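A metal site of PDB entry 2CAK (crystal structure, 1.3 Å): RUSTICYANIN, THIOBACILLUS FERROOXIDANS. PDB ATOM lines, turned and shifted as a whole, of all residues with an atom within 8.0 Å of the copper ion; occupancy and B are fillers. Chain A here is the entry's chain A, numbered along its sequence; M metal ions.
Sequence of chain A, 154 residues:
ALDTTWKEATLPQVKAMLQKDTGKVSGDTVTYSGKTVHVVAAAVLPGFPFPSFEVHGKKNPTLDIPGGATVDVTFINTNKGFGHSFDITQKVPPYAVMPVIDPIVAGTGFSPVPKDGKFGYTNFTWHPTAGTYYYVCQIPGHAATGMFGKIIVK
The backbone carbonyl oxygen (O) of His 142 sits at hydrogen-bond distance from the side-chain hydroxyl (OG1) of Thr 145, 3.1 Å away. OG of Ser 111 sits at hydrogen-bond distance from O of His 84 (2.8 Å). The backbone NH of Met 147 lies within hydrogen-bond range of the backbone carbonyl oxygen of His 142 (3.0 Å). N of Ile 139 sits close to SG of Cys 137 (3.4 Å). A ring nitrogen (ND1) of His 84 lies close to the side-chain sulfur of Met 147 (3.5 Å). NE2 of His 84 lies within hydrogen-bond range of ND2 of Asn 79, at 2.7 Å. The backbone NH (N) of Cys 137 is in hydrogen-bond range of the backbone carbonyl oxygen (O) of Met 147 (3.5 Å). SG of Cys 137 lies close to N of Ser 85, at 3.5 Å.
Residues that only touch the copper ion: Ile 139 (3.8 Å). Within 4 Å of the copper ion: His 84, Cys 137, Ile 139, His 142 and Met 147. The nearest printed residue that does not touch the copper ion is Ser 85 (4.8 Å).
The copper ion is bound by a ring nitrogen (ND1) of His 84. ND1 of His 142 is bound to the copper ion (2.1 Å). SG of Cys 137 is bound to the copper ion, 2.2 Å away. Slightly farther from the copper ion lies the side-chain sulfur (SD) of Met 147 (2.9 Å).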
ATOM      1  N   ALA A  43      -8.143  -0.623   3.637  1.00  0.00           N
ATOM      2  CA  ALA A  43      -8.466   0.212   4.781  1.00  0.00           C
ATOM      3  C   ALA A  43      -7.405   0.050   5.872  1.00  0.00           C
ATOM      4  O   ALA A  43      -7.304  -1.047   6.429  1.00  0.00           O
ATOM      5  CB  ALA A  43      -9.828  -0.125   5.361  1.00  0.00           C
ATOM      6  N   VAL A  44      -6.631   1.089   6.108  1.00  0.00           N
ATOM      7  CA  VAL A  44      -5.592   1.202   7.127  1.00  0.00           C
ATOM      8  C   VAL A  44      -4.620   0.012   7.119  1.00  0.00           C
ATOM      9  O   VAL A  44      -4.615  -0.889   7.936  1.00  0.00           O
ATOM     10  CB  VAL A  44      -6.158   1.425   8.543  1.00  0.00           C
ATOM     11  CG1 VAL A  44      -5.063   2.054   9.410  1.00  0.00           C
ATOM     12  CG2 VAL A  44      -7.348   2.356   8.536  1.00  0.00           C
ATOM     13  N   PHE A  50      -4.636   6.115  10.975  1.00  0.00           N
ATOM     14  CA  PHE A  50      -6.045   5.847  11.176  1.00  0.00           C
ATOM     15  C   PHE A  50      -6.824   7.172  11.142  1.00  0.00           C
ATOM     16  O   PHE A  50      -6.487   8.093  11.899  1.00  0.00           O
ATOM     17  CB  PHE A  50      -6.336   5.084  12.481  1.00  0.00           C
ATOM     18  CG  PHE A  50      -7.764   4.773  12.794  1.00  0.00           C
ATOM     19  CD1 PHE A  50      -8.565   5.682  13.470  1.00  0.00           C
ATOM     20  CD2 PHE A  50      -8.314   3.548  12.396  1.00  0.00           C
ATOM     21  CE1 PHE A  50      -9.853   5.416  13.690  1.00  0.00           C
ATOM     22  CE2 PHE A  50      -9.661   3.272  12.634  1.00  0.00           C
ATOM     23  CZ  PHE A  50     -10.388   4.202  13.304  1.00  0.00           C
ATOM     24  N   PRO A  51      -7.971   7.223  10.500  1.00  0.00           N
ATOM     25  CA  PRO A  51      -8.540   6.302   9.506  1.00  0.00           C
ATOM     26  C   PRO A  51      -8.164   6.781   8.093  1.00  0.00           C
ATOM     27  O   PRO A  51      -8.187   7.969   7.818  1.00  0.00           O
ATOM     28  CB  PRO A  51     -10.027   6.455   9.790  1.00  0.00           C
ATOM     29  CG  PRO A  51     -10.203   7.878  10.174  1.00  0.00           C
ATOM     30  CD  PRO A  51      -8.933   8.330  10.811  1.00  0.00           C
ATOM     31  N   SER A  52      -7.816   5.871   7.206  1.00  0.00           N
ATOM     32  CA  SER A  52      -7.371   6.197   5.872  1.00  0.00           C
ATOM     33  C   SER A  52      -7.543   4.999   4.938  1.00  0.00           C
ATOM     34  O   SER A  52      -7.593   3.880   5.423  1.00  0.00           O
ATOM     35  CB  SER A  52      -5.933   6.631   5.863  1.00  0.00           C
ATOM     36  OG  SER A  52      -5.016   5.630   6.146  1.00  0.00           O
ATOM     37  N   PHE A  53      -7.587   5.275   3.652  1.00  0.00           N
ATOM     38  CA  PHE A  53      -7.448   4.259   2.619  1.00  0.00           C
ATOM     39  C   PHE A  53      -6.063   4.324   1.994  1.00  0.00           C
ATOM     40  O   PHE A  53      -5.535   5.420   1.799  1.00  0.00           O
ATOM     41  CB  PHE A  53      -8.440   4.528   1.487  1.00  0.00           C
ATOM     42  CG  PHE A  53      -9.921   4.402   1.815  1.00  0.00           C
ATOM     43  CD1 PHE A  53     -10.493   3.150   1.991  1.00  0.00           C
ATOM     44  CD2 PHE A  53     -10.731   5.513   1.956  1.00  0.00           C
ATOM     45  CE1 PHE A  53     -11.830   3.038   2.226  1.00  0.00           C
ATOM     46  CE2 PHE A  53     -12.076   5.384   2.159  1.00  0.00           C
ATOM     47  CZ  PHE A  53     -12.646   4.152   2.330  1.00  0.00           C
ATOM     48  N   PHE A  75     -11.403  -4.275  -2.788  1.00  0.00           N
ATOM     49  CA  PHE A  75     -11.323  -3.590  -1.491  1.00  0.00           C
ATOM     50  C   PHE A  75     -11.049  -4.619  -0.400  1.00  0.00           C
ATOM     51  O   PHE A  75     -11.780  -5.620  -0.282  1.00  0.00           O
ATOM     52  CB  PHE A  75     -12.612  -2.829  -1.172  1.00  0.00           C
ATOM     53  CG  PHE A  75     -12.645  -2.197   0.204  1.00  0.00           C
ATOM     54  CD1 PHE A  75     -11.676  -1.311   0.619  1.00  0.00           C
ATOM     55  CD2 PHE A  75     -13.621  -2.542   1.093  1.00  0.00           C
ATOM     56  CE1 PHE A  75     -11.654  -0.778   1.909  1.00  0.00           C
ATOM     57  CE2 PHE A  75     -13.651  -2.034   2.339  1.00  0.00           C
ATOM     58  CZ  PHE A  75     -12.690  -1.156   2.763  1.00  0.00           C
ATOM     59  N   ASN A  77     -10.141  -5.060   3.820  1.00  0.00           N
ATOM     60  CA  ASN A  77     -10.126  -4.454   5.108  1.00  0.00           C
ATOM     61  C   ASN A  77      -9.046  -5.127   5.971  1.00  0.00           C
ATOM     62  O   ASN A  77      -9.237  -6.231   6.498  1.00  0.00           O
ATOM     63  CB  ASN A  77     -11.472  -4.539   5.839  1.00  0.00           C
ATOM     64  CG  ASN A  77     -11.440  -3.969   7.244  1.00  0.00           C
ATOM     65  OD1 ASN A  77     -12.274  -4.383   8.125  1.00  0.00           O
ATOM     66  ND2 ASN A  77     -10.542  -3.099   7.518  1.00  0.00           N
ATOM     67  N   ASN A  79      -7.767  -3.636   8.796  1.00  0.00           N
ATOM     68  CA  ASN A  79      -7.727  -2.928  10.088  1.00  0.00           C
ATOM     69  C   ASN A  79      -8.422  -3.703  11.163  1.00  0.00           C
ATOM     70  O   ASN A  79      -9.655  -3.794  11.188  1.00  0.00           O
ATOM     71  CB  ASN A  79      -8.333  -1.525   9.895  1.00  0.00           C
ATOM     72  CG  ASN A  79      -8.044  -0.611  11.076  1.00  0.00           C
ATOM     73  OD1 ASN A  79      -7.047  -0.667  11.845  1.00  0.00           O
ATOM     74  ND2 ASN A  79      -8.933   0.287  11.196  1.00  0.00           N
ATOM     75  N   PHE A  82     -12.359  -2.938  13.220  1.00  0.00           N
ATOM     76  CA  PHE A  82     -13.239  -2.032  12.509  1.00  0.00           C
ATOM     77  C   PHE A  82     -13.725  -2.661  11.219  1.00  0.00           C
ATOM     78  O   PHE A  82     -12.978  -3.334  10.554  1.00  0.00           O
ATOM     79  CB  PHE A  82     -12.522  -0.713  12.163  1.00  0.00           C
ATOM     80  CG  PHE A  82     -12.160   0.019  13.438  1.00  0.00           C
ATOM     81  CD1 PHE A  82     -10.958  -0.182  14.085  1.00  0.00           C
ATOM     82  CD2 PHE A  82     -13.079   0.880  13.995  1.00  0.00           C
ATOM     83  CE1 PHE A  82     -10.673   0.483  15.260  1.00  0.00           C
ATOM     84  CE2 PHE A  82     -12.781   1.594  15.166  1.00  0.00           C
ATOM     85  CZ  PHE A  82     -11.578   1.397  15.783  1.00  0.00           C
ATOM     86  N   GLY A  83     -14.967  -2.398  10.863  1.00  0.00           N
ATOM     87  CA  GLY A  83     -15.563  -2.849   9.620  1.00  0.00           C
ATOM     88  C   GLY A  83     -15.815  -1.814   8.563  1.00  0.00           C
ATOM     89  O   GLY A  83     -16.955  -1.535   8.143  1.00  0.00           O
ATOM     90  N   HIS A  84     -14.782  -1.224   8.030  1.00  0.00           N
ATOM     91  CA  HIS A  84     -14.833  -0.097   7.101  1.00  0.00           C
ATOM     92  C   HIS A  84     -15.541  -0.463   5.818  1.00  0.00           C
ATOM     93  O   HIS A  84     -15.566  -1.628   5.390  1.00  0.00           O
ATOM     94  CB  HIS A  84     -13.382   0.290   6.769  1.00  0.00           C
ATOM     95  CG  HIS A  84     -12.530   0.730   7.910  1.00  0.00           C
ATOM     96  ND1 HIS A  84     -12.592   1.968   8.518  1.00  0.00           N
ATOM     97  CD2 HIS A  84     -11.527   0.044   8.508  1.00  0.00           C
ATOM     98  CE1 HIS A  84     -11.647   1.986   9.444  1.00  0.00           C
ATOM     99  NE2 HIS A  84     -10.972   0.820   9.493  1.00  0.00           N
ATOM    100  N   SER A  85     -16.077   0.551   5.156  1.00  0.00           N
ATOM    101  CA  SER A  85     -16.686   0.375   3.847  1.00  0.00           C
ATOM    102  C   SER A  85     -15.931   1.180   2.794  1.00  0.00           C
ATOM    103  O   SER A  85     -15.087   2.015   3.114  1.00  0.00           O
ATOM    104  CB  SER A  85     -18.165   0.783   3.816  1.00  0.00           C
ATOM    105  OG  SER A  85     -18.341   2.183   3.929  1.00  0.00           O
ATOM    106  N   PHE A  86     -16.226   0.960   1.528  1.00  0.00           N
ATOM    107  CA  PHE A  86     -15.663   1.694   0.393  1.00  0.00           C
ATOM    108  C   PHE A  86     -16.841   2.033  -0.528  1.00  0.00           C
ATOM    109  O   PHE A  86     -17.373   1.162  -1.207  1.00  0.00           O
ATOM    110  CB  PHE A  86     -14.613   0.851  -0.331  1.00  0.00           C
ATOM    111  CG  PHE A  86     -13.895   1.558  -1.462  1.00  0.00           C
ATOM    112  CD1 PHE A  86     -12.619   2.092  -1.259  1.00  0.00           C
ATOM    113  CD2 PHE A  86     -14.428   1.717  -2.720  1.00  0.00           C
ATOM    114  CE1 PHE A  86     -11.958   2.752  -2.269  1.00  0.00           C
ATOM    115  CE2 PHE A  86     -13.737   2.394  -3.691  1.00  0.00           C
ATOM    116  CZ  PHE A  86     -12.505   2.912  -3.527  1.00  0.00           C
ATOM    117  N   PHE A 110     -20.657  -2.570   4.941  1.00  0.00           N
ATOM    118  CA  PHE A 110     -19.605  -2.678   5.947  1.00  0.00           C
ATOM    119  C   PHE A 110     -18.920  -4.035   5.852  1.00  0.00           C
ATOM    120  O   PHE A 110     -19.546  -5.084   5.682  1.00  0.00           O
ATOM    121  CB  PHE A 110     -20.204  -2.434   7.351  1.00  0.00           C
ATOM    122  CG  PHE A 110     -20.742  -1.021   7.532  1.00  0.00           C
ATOM    123  CD1 PHE A 110     -19.905   0.060   7.539  1.00  0.00           C
ATOM    124  CD2 PHE A 110     -22.093  -0.803   7.668  1.00  0.00           C
ATOM    125  CE1 PHE A 110     -20.382   1.363   7.629  1.00  0.00           C
ATOM    126  CE2 PHE A 110     -22.571   0.489   7.760  1.00  0.00           C
ATOM    127  CZ  PHE A 110     -21.723   1.603   7.737  1.00  0.00           C
ATOM    128  N   SER A 111     -17.574  -4.003   5.933  1.00  0.00           N
ATOM    129  CA  SER A 111     -16.757  -5.194   5.768  1.00  0.00           C
ATOM    130  C   SER A 111     -16.690  -5.999   7.056  1.00  0.00           C
ATOM    131  O   SER A 111     -16.872  -5.453   8.179  1.00  0.00           O
ATOM    132  CB  SER A 111     -15.364  -4.824   5.383  1.00  0.00           C
ATOM    133  OG  SER A 111     -14.674  -4.044   6.358  1.00  0.00           O
ATOM    134  N   VAL A 136     -15.416   7.046  -0.025  1.00  0.00           N
ATOM    135  CA  VAL A 136     -15.603   7.360   1.379  1.00  0.00           C
ATOM    136  C   VAL A 136     -15.864   6.086   2.158  1.00  0.00           C
ATOM    137  O   VAL A 136     -16.379   5.109   1.605  1.00  0.00           O
ATOM    138  CB  VAL A 136     -16.742   8.397   1.622  1.00  0.00           C
ATOM    139  CG1 VAL A 136     -16.637   9.595   0.710  1.00  0.00           C
ATOM    140  CG2 VAL A 136     -18.127   7.775   1.470  1.00  0.00           C
ATOM    141  N   CYS A 137     -15.604   6.107   3.443  1.00  0.00           N
ATOM    142  CA  CYS A 137     -16.062   5.135   4.400  1.00  0.00           C
ATOM    143  C   CYS A 137     -17.321   5.678   5.119  1.00  0.00           C
ATOM    144  O   CYS A 137     -17.335   6.875   5.452  1.00  0.00           O
ATOM    145  CB  CYS A 137     -15.005   4.803   5.430  1.00  0.00           C
ATOM    146  SG  CYS A 137     -15.532   3.616   6.716  1.00  0.00           S
ATOM    147  N   GLN A 138     -18.304   4.790   5.337  1.00  0.00           N
ATOM    148  CA  GLN A 138     -19.540   5.202   5.992  1.00  0.00           C
ATOM    149  C   GLN A 138     -19.567   5.021   7.511  1.00  0.00           C
ATOM    150  O   GLN A 138     -20.579   5.399   8.126  1.00  0.00           O
ATOM    151  CB  GLN A 138     -20.756   4.464   5.393  1.00  0.00           C
ATOM    152  CG  GLN A 138     -21.065   4.914   3.982  1.00  0.00           C
ATOM    153  CD  GLN A 138     -22.453   4.383   3.606  1.00  0.00           C
ATOM    154  OE1 GLN A 138     -22.747   3.290   3.143  1.00  0.00           O
ATOM    155  NE2 GLN A 138     -23.354   5.261   3.985  1.00  0.00           N
ATOM    156  N   ILE A 139     -18.530   4.456   8.117  1.00  0.00           N
ATOM    157  CA  ILE A 139     -18.563   4.343   9.576  1.00  0.00           C
ATOM    158  C   ILE A 139     -18.689   5.720  10.174  1.00  0.00           C
ATOM    159  O   ILE A 139     -17.897   6.592   9.766  1.00  0.00           O
ATOM    160  CB  ILE A 139     -17.357   3.621  10.158  1.00  0.00           C
ATOM    161  CG1 ILE A 139     -17.315   2.140   9.776  1.00  0.00           C
ATOM    162  CG2 ILE A 139     -17.338   3.738  11.693  1.00  0.00           C
ATOM    163  CD1 ILE A 139     -16.100   1.357  10.329  1.00  0.00           C
ATOM    164  N   PRO A 140     -19.630   5.981  11.063  1.00  0.00           N
ATOM    165  CA  PRO A 140     -19.747   7.374  11.606  1.00  0.00           C
ATOM    166  C   PRO A 140     -18.449   7.940  12.128  1.00  0.00           C
ATOM    167  O   PRO A 140     -17.703   7.314  12.869  1.00  0.00           O
ATOM    168  CB  PRO A 140     -20.781   7.175  12.737  1.00  0.00           C
ATOM    169  CG  PRO A 140     -21.690   6.102  12.170  1.00  0.00           C
ATOM    170  CD  PRO A 140     -20.705   5.125  11.545  1.00  0.00           C
ATOM    171  N   GLY A 141     -18.121   9.134  11.651  1.00  0.00           N
ATOM    172  CA  GLY A 141     -16.934   9.849  12.008  1.00  0.00           C
ATOM    173  C   GLY A 141     -15.755   9.680  11.093  1.00  0.00           C
ATOM    174  O   GLY A 141     -14.839  10.497  11.111  1.00  0.00           O
ATOM    175  N   HIS A 142     -15.684   8.583  10.299  1.00  0.00           N
ATOM    176  CA  HIS A 142     -14.440   8.306   9.605  1.00  0.00           C
ATOM    177  C   HIS A 142     -14.208   9.272   8.434  1.00  0.00           C
ATOM    178  O   HIS A 142     -13.074   9.777   8.326  1.00  0.00           O
ATOM    179  CB  HIS A 142     -14.417   6.848   9.137  1.00  0.00           C
ATOM    180  CG  HIS A 142     -14.166   5.870  10.260  1.00  0.00           C
ATOM    181  ND1 HIS A 142     -13.846   4.548  10.017  1.00  0.00           N
ATOM    182  CD2 HIS A 142     -14.208   6.071  11.601  1.00  0.00           C
ATOM    183  CE1 HIS A 142     -13.702   3.994  11.222  1.00  0.00           C
ATOM    184  NE2 HIS A 142     -13.911   4.880  12.199  1.00  0.00           N
ATOM    185  N   ALA A 143     -15.194   9.482   7.577  1.00  0.00           N
ATOM    186  CA  ALA A 143     -15.038  10.475   6.525  1.00  0.00           C
ATOM    187  C   ALA A 143     -14.748  11.883   7.051  1.00  0.00           C
ATOM    188  O   ALA A 143     -13.969  12.613   6.430  1.00  0.00           O
ATOM    189  CB  ALA A 143     -16.234  10.436   5.571  1.00  0.00           C
ATOM    190  N   THR A 145     -13.136  12.646   9.571  1.00  0.00           N
ATOM    191  CA  THR A 145     -11.790  12.717  10.080  1.00  0.00           C
ATOM    192  C   THR A 145     -10.768  12.328   9.037  1.00  0.00           C
ATOM    193  O   THR A 145      -9.610  12.080   9.421  1.00  0.00           O
ATOM    194  CB  THR A 145     -11.685  11.866  11.363  1.00  0.00           C
ATOM    195  OG1 THR A 145     -12.133  10.542  11.161  1.00  0.00           O
ATOM    196  CG2 THR A 145     -12.676  12.411  12.382  1.00  0.00           C
ATOM    197  N   MET A 147     -11.098   9.908   6.121  1.00  0.00           N
ATOM    198  CA  MET A 147     -11.084   8.671   5.361  1.00  0.00           C
ATOM    199  C   MET A 147     -11.879   8.832   4.084  1.00  0.00           C
ATOM    200  O   MET A 147     -13.048   8.386   3.990  1.00  0.00           O
ATOM    201  CB  MET A 147     -11.625   7.509   6.227  1.00  0.00           C
ATOM    202  CG  MET A 147     -11.355   6.147   5.623  1.00  0.00           C
ATOM    203  SD  MET A 147     -11.597   4.819   6.836  1.00  0.00           S
ATOM    204  CE  MET A 147     -11.074   3.391   5.809  1.00  0.00           C
HETATM  205 CU    CU M   1     -13.861   3.554   8.189  1.00  0.00          CU
